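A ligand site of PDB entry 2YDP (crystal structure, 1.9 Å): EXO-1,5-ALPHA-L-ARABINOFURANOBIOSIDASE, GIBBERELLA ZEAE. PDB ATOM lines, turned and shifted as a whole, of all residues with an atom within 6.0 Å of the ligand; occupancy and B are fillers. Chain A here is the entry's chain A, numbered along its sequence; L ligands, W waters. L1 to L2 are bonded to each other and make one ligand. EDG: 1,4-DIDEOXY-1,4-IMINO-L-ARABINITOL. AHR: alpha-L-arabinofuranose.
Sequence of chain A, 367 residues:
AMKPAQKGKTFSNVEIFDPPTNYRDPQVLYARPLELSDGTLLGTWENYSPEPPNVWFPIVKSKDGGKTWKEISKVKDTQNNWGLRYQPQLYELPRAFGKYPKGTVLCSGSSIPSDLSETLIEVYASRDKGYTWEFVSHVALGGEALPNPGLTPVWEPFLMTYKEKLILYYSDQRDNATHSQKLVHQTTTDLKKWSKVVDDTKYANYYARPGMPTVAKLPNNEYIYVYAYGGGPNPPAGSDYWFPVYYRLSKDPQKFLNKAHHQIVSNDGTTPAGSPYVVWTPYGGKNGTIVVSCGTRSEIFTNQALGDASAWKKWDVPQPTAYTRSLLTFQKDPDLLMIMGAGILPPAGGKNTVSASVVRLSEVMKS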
ATOM      1  N   PRO A  26      21.667  -0.659  -0.477  1.00  0.00           N
ATOM      2  CA  PRO A  26      20.617  -0.796  -1.490  1.00  0.00           C
ATOM      3  C   PRO A  26      20.200   0.469  -2.212  1.00  0.00           C
ATOM      4  O   PRO A  26      19.217   0.426  -2.916  1.00  0.00           O
ATOM      5  CB  PRO A  26      19.412  -1.349  -0.682  1.00  0.00           C
ATOM      6  CG  PRO A  26      19.529  -0.705   0.658  1.00  0.00           C
ATOM      7  CD  PRO A  26      21.092  -0.553   0.883  1.00  0.00           C
ATOM      8  N   LEU A  29      15.954   2.982   0.543  1.00  0.00           N
ATOM      9  CA  LEU A  29      15.203   2.008   1.360  1.00  0.00           C
ATOM     10  C   LEU A  29      14.366   2.817   2.320  1.00  0.00           C
ATOM     11  O   LEU A  29      14.675   3.975   2.548  1.00  0.00           O
ATOM     12  CB  LEU A  29      16.182   1.152   2.175  1.00  0.00           C
ATOM     13  CG  LEU A  29      15.727  -0.174   2.779  1.00  0.00           C
ATOM     14  CD1 LEU A  29      15.633  -1.247   1.668  1.00  0.00           C
ATOM     15  CD2 LEU A  29      16.716  -0.603   3.854  1.00  0.00           C
ATOM     16  N   TYR A  30      13.332   2.198   2.904  1.00  0.00           N
ATOM     17  CA  TYR A  30      12.661   2.735   4.095  1.00  0.00           C
ATOM     18  C   TYR A  30      11.935   4.059   3.807  1.00  0.00           C
ATOM     19  O   TYR A  30      12.247   5.101   4.391  1.00  0.00           O
ATOM     20  CB  TYR A  30      13.709   2.922   5.217  1.00  0.00           C
ATOM     21  CG  TYR A  30      13.176   2.766   6.632  1.00  0.00           C
ATOM     22  CD1 TYR A  30      12.321   3.717   7.191  1.00  0.00           C
ATOM     23  CD2 TYR A  30      13.553   1.682   7.405  1.00  0.00           C
ATOM     24  CE1 TYR A  30      11.858   3.564   8.497  1.00  0.00           C
ATOM     25  CE2 TYR A  30      13.078   1.513   8.690  1.00  0.00           C
ATOM     26  CZ  TYR A  30      12.230   2.456   9.218  1.00  0.00           C
ATOM     27  OH  TYR A  30      11.806   2.270  10.512  1.00  0.00           O
ATOM     28  N   GLU A  46      15.768   6.485   3.414  1.00  0.00           N
ATOM     29  CA  GLU A  46      17.187   6.345   3.584  1.00  0.00           C
ATOM     30  C   GLU A  46      17.813   6.478   2.205  1.00  0.00           C
ATOM     31  O   GLU A  46      17.482   5.765   1.272  1.00  0.00           O
ATOM     32  CB  GLU A  46      17.546   4.970   4.145  1.00  0.00           C
ATOM     33  CG  GLU A  46      16.993   4.676   5.554  1.00  0.00           C
ATOM     34  CD  GLU A  46      17.212   3.212   5.937  1.00  0.00           C
ATOM     35  OE1 GLU A  46      17.668   2.411   5.086  1.00  0.00           O
ATOM     36  OE2 GLU A  46      16.887   2.839   7.087  1.00  0.00           O
ATOM     37  N   TYR A  48      21.275   6.402   0.222  1.00  0.00           N
ATOM     38  CA  TYR A  48      22.615   5.836   0.386  1.00  0.00           C
ATOM     39  C   TYR A  48      23.593   6.472  -0.627  1.00  0.00           C
ATOM     40  O   TYR A  48      24.227   5.770  -1.430  1.00  0.00           O
ATOM     41  CB  TYR A  48      22.578   4.322   0.206  1.00  0.00           C
ATOM     42  CG  TYR A  48      21.916   3.573   1.315  1.00  0.00           C
ATOM     43  CD1 TYR A  48      20.517   3.636   1.503  1.00  0.00           C
ATOM     44  CD2 TYR A  48      22.661   2.777   2.171  1.00  0.00           C
ATOM     45  CE1 TYR A  48      19.906   2.931   2.526  1.00  0.00           C
ATOM     46  CE2 TYR A  48      22.038   2.043   3.186  1.00  0.00           C
ATOM     47  CZ  TYR A  48      20.669   2.145   3.358  1.00  0.00           C
ATOM     48  OH  TYR A  48      20.084   1.438   4.376  1.00  0.00           O
ATOM     49  N   TYR A  86      19.734   6.066   8.919  1.00  0.00           N
ATOM     50  CA  TYR A  86      18.753   4.984   8.913  1.00  0.00           C
ATOM     51  C   TYR A  86      17.388   5.385   9.432  1.00  0.00           C
ATOM     52  O   TYR A  86      17.292   6.202  10.364  1.00  0.00           O
ATOM     53  CB  TYR A  86      19.210   3.812   9.784  1.00  0.00           C
ATOM     54  CG  TYR A  86      20.262   2.854   9.197  1.00  0.00           C
ATOM     55  CD1 TYR A  86      20.641   2.908   7.846  1.00  0.00           C
ATOM     56  CD2 TYR A  86      20.827   1.859  10.001  1.00  0.00           C
ATOM     57  CE1 TYR A  86      21.611   2.012   7.327  1.00  0.00           C
ATOM     58  CE2 TYR A  86      21.797   0.981   9.507  1.00  0.00           C
ATOM     59  CZ  TYR A  86      22.183   1.073   8.173  1.00  0.00           C
ATOM     60  OH  TYR A  86      23.092   0.150   7.686  1.00  0.00           O
ATOM     61  N   GLN A  87      16.341   4.758   8.883  1.00  0.00           N
ATOM     62  CA  GLN A  87      15.025   4.703   9.563  1.00  0.00           C
ATOM     63  C   GLN A  87      14.357   6.033   9.875  1.00  0.00           C
ATOM     64  O   GLN A  87      14.002   6.307  11.049  1.00  0.00           O
ATOM     65  CB  GLN A  87      15.171   3.893  10.875  1.00  0.00           C
ATOM     66  CG  GLN A  87      15.594   2.423  10.591  1.00  0.00           C
ATOM     67  CD  GLN A  87      16.736   1.908  11.464  1.00  0.00           C
ATOM     68  OE1 GLN A  87      16.973   2.401  12.578  1.00  0.00           O
ATOM     69  NE2 GLN A  87      17.445   0.886  10.962  1.00  0.00           N
ATOM     70  N   ALA A 145      25.824  -0.549  14.634  1.00  0.00           N
ATOM     71  CA  ALA A 145      24.618  -0.598  13.809  1.00  0.00           C
ATOM     72  C   ALA A 145      24.561  -1.839  12.931  1.00  0.00           C
ATOM     73  O   ALA A 145      24.476  -1.739  11.696  1.00  0.00           O
ATOM     74  CB  ALA A 145      24.487   0.677  13.000  1.00  0.00           C
ATOM     75  N   LEU A 146      24.619  -3.008  13.565  1.00  0.00           N
ATOM     76  CA  LEU A 146      24.317  -4.307  12.919  1.00  0.00           C
ATOM     77  C   LEU A 146      23.314  -5.095  13.745  1.00  0.00           C
ATOM     78  O   LEU A 146      23.398  -5.124  14.982  1.00  0.00           O
ATOM     79  CB  LEU A 146      25.597  -5.151  12.677  1.00  0.00           C
ATOM     80  CG  LEU A 146      26.713  -4.535  11.837  1.00  0.00           C
ATOM     81  CD1 LEU A 146      28.000  -5.374  11.958  1.00  0.00           C
ATOM     82  CD2 LEU A 146      26.333  -4.423  10.373  1.00  0.00           C
ATOM     83  N   PRO A 147      22.334  -5.727  13.072  1.00  0.00           N
ATOM     84  CA  PRO A 147      21.289  -6.402  13.826  1.00  0.00           C
ATOM     85  C   PRO A 147      21.720  -7.804  14.289  1.00  0.00           C
ATOM     86  O   PRO A 147      21.092  -8.782  13.895  1.00  0.00           O
ATOM     87  CB  PRO A 147      20.136  -6.488  12.818  1.00  0.00           C
ATOM     88  CG  PRO A 147      20.863  -6.632  11.473  1.00  0.00           C
ATOM     89  CD  PRO A 147      22.078  -5.719  11.614  1.00  0.00           C
ATOM     90  N   TRP A 155      17.205   1.347  17.094  1.00  0.00           N
ATOM     91  CA  TRP A 155      16.701   1.462  15.728  1.00  0.00           C
ATOM     92  C   TRP A 155      15.240   1.921  15.649  1.00  0.00           C
ATOM     93  O   TRP A 155      14.488   1.742  16.598  1.00  0.00           O
ATOM     94  CB  TRP A 155      16.692   0.084  15.057  1.00  0.00           C
ATOM     95  CG  TRP A 155      17.788  -0.916  15.263  1.00  0.00           C
ATOM     96  CD1 TRP A 155      17.811  -1.896  16.167  1.00  0.00           C
ATOM     97  CD2 TRP A 155      18.940  -1.111  14.420  1.00  0.00           C
ATOM     98  NE1 TRP A 155      18.899  -2.714  15.967  1.00  0.00           N
ATOM     99  CE2 TRP A 155      19.621  -2.238  14.901  1.00  0.00           C
ATOM    100  CE3 TRP A 155      19.455  -0.437  13.296  1.00  0.00           C
ATOM    101  CZ2 TRP A 155      20.789  -2.732  14.309  1.00  0.00           C
ATOM    102  CZ3 TRP A 155      20.645  -0.906  12.733  1.00  0.00           C
ATOM    103  CH2 TRP A 155      21.292  -2.041  13.227  1.00  0.00           C
ATOM    104  N   GLU A 156      14.841   2.412  14.460  1.00  0.00           N
ATOM    105  CA  GLU A 156      13.448   2.327  13.989  1.00  0.00           C
ATOM    106  C   GLU A 156      12.419   3.136  14.836  1.00  0.00           C
ATOM    107  O   GLU A 156      11.445   2.569  15.341  1.00  0.00           O
ATOM    108  CB  GLU A 156      13.032   0.833  13.897  1.00  0.00           C
ATOM    109  CG  GLU A 156      13.733   0.077  12.753  1.00  0.00           C
ATOM    110  CD  GLU A 156      14.072  -1.398  13.022  1.00  0.00           C
ATOM    111  OE1 GLU A 156      13.829  -1.936  14.113  1.00  0.00           O
ATOM    112  OE2 GLU A 156      14.649  -2.001  12.090  1.00  0.00           O
ATOM    113  N   SER A 171      13.198   0.196  18.657  1.00  0.00           N
ATOM    114  CA  SER A 171      13.770  -1.146  18.880  1.00  0.00           C
ATOM    115  C   SER A 171      15.086  -1.009  19.613  1.00  0.00           C
ATOM    116  O   SER A 171      15.869  -0.099  19.305  1.00  0.00           O
ATOM    117  CB  SER A 171      14.057  -1.853  17.551  1.00  0.00           C
ATOM    118  OG  SER A 171      12.899  -1.898  16.746  1.00  0.00           O
ATOM    119  N   GLN A 173      18.546  -2.915  21.454  1.00  0.00           N
ATOM    120  CA  GLN A 173      19.440  -4.052  21.715  1.00  0.00           C
ATOM    121  C   GLN A 173      20.334  -3.819  22.940  1.00  0.00           C
ATOM    122  O   GLN A 173      21.242  -4.614  23.209  1.00  0.00           O
ATOM    123  CB  GLN A 173      20.334  -4.317  20.510  1.00  0.00           C
ATOM    124  CG  GLN A 173      19.579  -4.753  19.262  1.00  0.00           C
ATOM    125  CD  GLN A 173      20.479  -5.333  18.170  1.00  0.00           C
ATOM    126  OE1 GLN A 173      20.282  -5.055  16.987  1.00  0.00           O
ATOM    127  NE2 GLN A 173      21.455  -6.147  18.555  1.00  0.00           N
ATOM    128  N   GLN A 181      17.105  -8.353  21.139  1.00  0.00           N
ATOM    129  CA  GLN A 181      16.495  -7.040  20.949  1.00  0.00           C
ATOM    130  C   GLN A 181      15.154  -7.049  21.698  1.00  0.00           C
ATOM    131  O   GLN A 181      14.540  -8.118  21.908  1.00  0.00           O
ATOM    132  CB  GLN A 181      16.325  -6.793  19.436  1.00  0.00           C
ATOM    133  CG  GLN A 181      15.835  -5.398  19.101  1.00  0.00           C
ATOM    134  CD  GLN A 181      15.800  -5.177  17.615  1.00  0.00           C
ATOM    135  OE1 GLN A 181      16.768  -4.712  17.020  1.00  0.00           O
ATOM    136  NE2 GLN A 181      14.667  -5.478  17.021  1.00  0.00           N
ATOM    137  N   ARG A 209      13.860 -11.519  18.786  1.00  0.00           N
ATOM    138  CA  ARG A 209      14.109 -10.159  18.358  1.00  0.00           C
ATOM    139  C   ARG A 209      12.835  -9.464  17.847  1.00  0.00           C
ATOM    140  O   ARG A 209      12.703  -9.231  16.645  1.00  0.00           O
ATOM    141  CB  ARG A 209      15.193 -10.161  17.262  1.00  0.00           C
ATOM    142  CG  ARG A 209      16.557 -10.618  17.732  1.00  0.00           C
ATOM    143  CD  ARG A 209      17.524 -10.700  16.534  1.00  0.00           C
ATOM    144  NE  ARG A 209      17.745  -9.397  15.895  1.00  0.00           N
ATOM    145  CZ  ARG A 209      18.532  -8.435  16.392  1.00  0.00           C
ATOM    146  NH1 ARG A 209      19.135  -8.612  17.569  1.00  0.00           N
ATOM    147  NH2 ARG A 209      18.675  -7.283  15.722  1.00  0.00           N
ATOM    148  N   PRO A 210      11.878  -9.173  18.749  1.00  0.00           N
ATOM    149  CA  PRO A 210      10.756  -8.343  18.353  1.00  0.00           C
ATOM    150  C   PRO A 210      11.300  -7.024  17.831  1.00  0.00           C
ATOM    151  O   PRO A 210      12.267  -6.482  18.408  1.00  0.00           O
ATOM    152  CB  PRO A 210      10.023  -8.106  19.674  1.00  0.00           C
ATOM    153  CG  PRO A 210      11.063  -8.336  20.740  1.00  0.00           C
ATOM    154  CD  PRO A 210      11.860  -9.474  20.185  1.00  0.00           C
ATOM    155  N   GLY A 211      10.747  -6.526  16.732  1.00  0.00           N
ATOM    156  CA  GLY A 211      11.318  -5.289  16.093  1.00  0.00           C
ATOM    157  C   GLY A 211      10.315  -4.509  15.260  1.00  0.00           C
ATOM    158  O   GLY A 211       9.210  -5.026  14.976  1.00  0.00           O
ATOM    159  N   MET A 212      10.660  -3.258  14.916  1.00  0.00           N
ATOM    160  CA  MET A 212       9.926  -2.392  13.950  1.00  0.00           C
ATOM    161  C   MET A 212       8.480  -2.084  14.366  1.00  0.00           C
ATOM    162  O   MET A 212       7.514  -2.528  13.720  1.00  0.00           O
ATOM    163  CB  MET A 212       9.963  -3.015  12.545  1.00  0.00           C
ATOM    164  CG  MET A 212      11.374  -3.581  12.229  1.00  0.00           C
ATOM    165  SD  MET A 212      11.732  -4.047  10.536  1.00  0.00           S
ATOM    166  CE  MET A 212      11.825  -2.407   9.790  1.00  0.00           C
ATOM    167  N   PHE A 243      10.224 -13.811  10.947  1.00  0.00           N
ATOM    168  CA  PHE A 243       9.770 -12.561  11.539  1.00  0.00           C
ATOM    169  C   PHE A 243       8.256 -12.354  11.404  1.00  0.00           C
ATOM    170  O   PHE A 243       7.820 -11.354  10.829  1.00  0.00           O
ATOM    171  CB  PHE A 243      10.536 -11.382  10.882  1.00  0.00           C
ATOM    172  CG  PHE A 243      12.038 -11.471  11.048  1.00  0.00           C
ATOM    173  CD1 PHE A 243      12.823 -12.199  10.151  1.00  0.00           C
ATOM    174  CD2 PHE A 243      12.663 -10.822  12.123  1.00  0.00           C
ATOM    175  CE1 PHE A 243      14.207 -12.264  10.301  1.00  0.00           C
ATOM    176  CE2 PHE A 243      14.035 -10.907  12.287  1.00  0.00           C
ATOM    177  CZ  PHE A 243      14.818 -11.624  11.378  1.00  0.00           C
ATOM    178  N   TYR A 323      10.615  -3.646   1.670  1.00  0.00           N
ATOM    179  CA  TYR A 323      11.022  -3.596   3.096  1.00  0.00           C
ATOM    180  C   TYR A 323      10.372  -2.373   3.762  1.00  0.00           C
ATOM    181  O   TYR A 323      10.479  -1.238   3.200  1.00  0.00           O
ATOM    182  CB  TYR A 323      12.532  -3.472   3.155  1.00  0.00           C
ATOM    183  CG  TYR A 323      13.106  -3.456   4.558  1.00  0.00           C
ATOM    184  CD1 TYR A 323      13.088  -4.623   5.345  1.00  0.00           C
ATOM    185  CD2 TYR A 323      13.685  -2.295   5.093  1.00  0.00           C
ATOM    186  CE1 TYR A 323      13.607  -4.604   6.665  1.00  0.00           C
ATOM    187  CE2 TYR A 323      14.201  -2.274   6.399  1.00  0.00           C
ATOM    188  CZ  TYR A 323      14.178  -3.438   7.159  1.00  0.00           C
ATOM    189  OH  TYR A 323      14.708  -3.414   8.426  1.00  0.00           O
ATOM    190  N   LEU A 345      15.784  -5.040   0.856  1.00  0.00           N
ATOM    191  CA  LEU A 345      17.037  -5.072   1.626  1.00  0.00           C
ATOM    192  C   LEU A 345      18.201  -5.432   0.702  1.00  0.00           C
ATOM    193  O   LEU A 345      17.985  -6.119  -0.310  1.00  0.00           O
ATOM    194  CB  LEU A 345      16.927  -6.149   2.726  1.00  0.00           C
ATOM    195  CG  LEU A 345      16.157  -5.718   3.969  1.00  0.00           C
ATOM    196  CD1 LEU A 345      15.753  -6.958   4.777  1.00  0.00           C
ATOM    197  CD2 LEU A 345      17.016  -4.728   4.826  1.00  0.00           C
ATOM    198  N   PRO A 346      19.414  -4.952   1.032  1.00  0.00           N
ATOM    199  CA  PRO A 346      20.581  -5.366   0.240  1.00  0.00           C
ATOM    200  C   PRO A 346      20.767  -6.898   0.324  1.00  0.00           C
ATOM    201  O   PRO A 346      20.445  -7.490   1.337  1.00  0.00           O
ATOM    202  CB  PRO A 346      21.766  -4.631   0.882  1.00  0.00           C
ATOM    203  CG  PRO A 346      21.326  -4.142   2.224  1.00  0.00           C
ATOM    204  CD  PRO A 346      19.770  -4.113   2.200  1.00  0.00           C
HETATM  205  O2' EDG L   1      14.117  -4.499  14.315  1.00  0.00           O
HETATM  206  C2' EDG L   1      15.147  -5.232  13.614  1.00  0.00           C
HETATM  207  C1' EDG L   1      14.729  -5.419  12.152  1.00  0.00           C
HETATM  208  N4' EDG L   1      15.638  -4.570  11.411  1.00  0.00           N
HETATM  209  C3' EDG L   1      16.438  -4.420  13.575  1.00  0.00           C
HETATM  210  O3' EDG L   1      17.403  -4.981  14.487  1.00  0.00           O
HETATM  211  C4' EDG L   1      16.904  -4.487  12.133  1.00  0.00           C
HETATM  212  C5' EDG L   1      17.752  -3.283  11.746  1.00  0.00           C
HETATM  213  O5' EDG L   1      18.461  -3.579  10.539  1.00  0.00           O
HETATM  214  O5  AHR L   2      17.062   0.384   7.935  1.00  0.00           O
HETATM  215  C5  AHR L   2      18.313  -0.103   7.495  1.00  0.00           C
HETATM  216  C4  AHR L   2      18.496  -1.517   8.022  1.00  0.00           C
HETATM  217  O4  AHR L   2      18.596  -1.496   9.451  1.00  0.00           O
HETATM  218  C3  AHR L   2      19.824  -2.190   7.638  1.00  0.00           C
HETATM  219  O3  AHR L   2      19.863  -2.677   6.285  1.00  0.00           O
HETATM  220  C2  AHR L   2      19.913  -3.328   8.640  1.00  0.00           C
HETATM  221  O2  AHR L   2      21.279  -3.703   8.887  1.00  0.00           O
HETATM  222  C1  AHR L   2      19.310  -2.670   9.868  1.00  0.00           C
HETATM  223  O   HOH W   1      13.752  -8.061  14.452  1.00  0.00           O
HETATM  224  O   HOH W   2      21.443  -6.185   8.186  1.00  0.00           O
HETATM  225  O   HOH W   3      16.255  -5.976   8.949  1.00  0.00           O
HETATM  226  O   HOH W   4      15.107  -1.202   9.451  1.00  0.00           O
HETATM  227  O   HOH W   5      20.975  -5.240   5.735  1.00  0.00           O
HETATM  228  O   HOH W   6      23.495  -2.105   9.143  1.00  0.00           O
HETATM  229  O   HOH W   7      20.751  -1.241   4.427  1.00  0.00           O
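Water W7 lies within hydrogen-bond range of O3 of AHR L2 (2.5 Å) and OH of Tyr 48 (2.8 Å). Water W6 lies within hydrogen-bond range of OH of Tyr 86 (2.7 Å), O2 of AHR L2 (2.7 Å) and O of Ala 145 (2.8 Å). Water W3 bridges N4' of EDG L1 (2.9 Å) and OH of Tyr 323 (3.0 Å). Water W4 lies within hydrogen-bond range of the side-chain hydroxyl (OH) of Tyr 323 (2.5 Å), the side-chain carboxylate (OE2) of Glu 156 (2.8 Å), an oxygen (O5) of AHR L2 (2.9 Å) and the side-chain amide nitrogen (NE2) of Gln 87 (3.5 Å).
The side-chain carboxylate of Glu 46 sits at hydrogen-bond distance from the side-chain hydroxyl of Tyr 48, 2.7 Å away. The side-chain amide oxygen (OE1) of Gln 87 lies within hydrogen-bond range of the backbone NH (N) of Glu 156 (2.8 Å). O of Leu 29 sits at hydrogen-bond distance from N of Glu 46. The side-chain amide oxygen of Gln 173 lies within hydrogen-bond range of the indole nitrogen of Trp 155 (2.9 Å). The side-chain amide oxygen (OE1) of Gln 181 is in hydrogen-bond range of the indole nitrogen (NE1) of Trp 155, at 3.1 Å. The side-chain hydroxyl (OH) of Tyr 323 lies close to the side-chain sulfur (SD) of Met 212. NE2 of Gln 181 is in hydrogen-bond range of O of Pro 210 (2.9 Å). NH2 of Arg 209 sits at hydrogen-bond distance from OE1 of Gln 173 (3.0 Å).
The side-chain hydroxyl (OH) of Tyr 323 sits at hydrogen-bond distance from a nitrogen (N4') of EDG L1. The side-chain amide nitrogen of Gln 87 lies within hydrogen-bond range of an oxygen (O4) of AHR L2, 3.0 Å away. The indole nitrogen (NE1) of Trp 155 is in hydrogen-bond range of an oxygen (O3') of EDG L1, 3.1 Å away. The side-chain amide oxygen of Gln 181 lies within hydrogen-bond range of an oxygen (O3') of EDG L1, at 2.6 Å. The side-chain carboxylate of Glu 156 is in salt-bridge range of a nitrogen (N4') of EDG L1, 2.8 Å away. The side-chain carboxylate (OE2) of Glu 46 sits at hydrogen-bond distance from an oxygen (O5) of AHR L2 (2.6 Å). An oxygen (O3') of EDG L1 sits at hydrogen-bond distance from the guanidinium group (NH2) of Arg 209, at 2.9 Å.
Residues that only touch the ligand: Tyr 30 (3.8 Å), Tyr 48 (3.9 Å), Tyr 86 (3.8 Å), Pro 147 (3.5 Å), Ser 171 (3.8 Å), Gln 173 (3.8 Å), Gly 211 (3.4 Å), Met 212 (3.6 Å) and Leu 345 (3.8 Å). Hydrophobic or aromatic side chains that line the ligand: Tyr 30, Tyr 86, Pro 147, Trp 155, Met 212 and Leu 345. Along chain A the residues within 4 Å of the ligand span positions 30 to 345. The nearest printed residue that does not touch the ligand is Leu 29 (4.01 Å).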
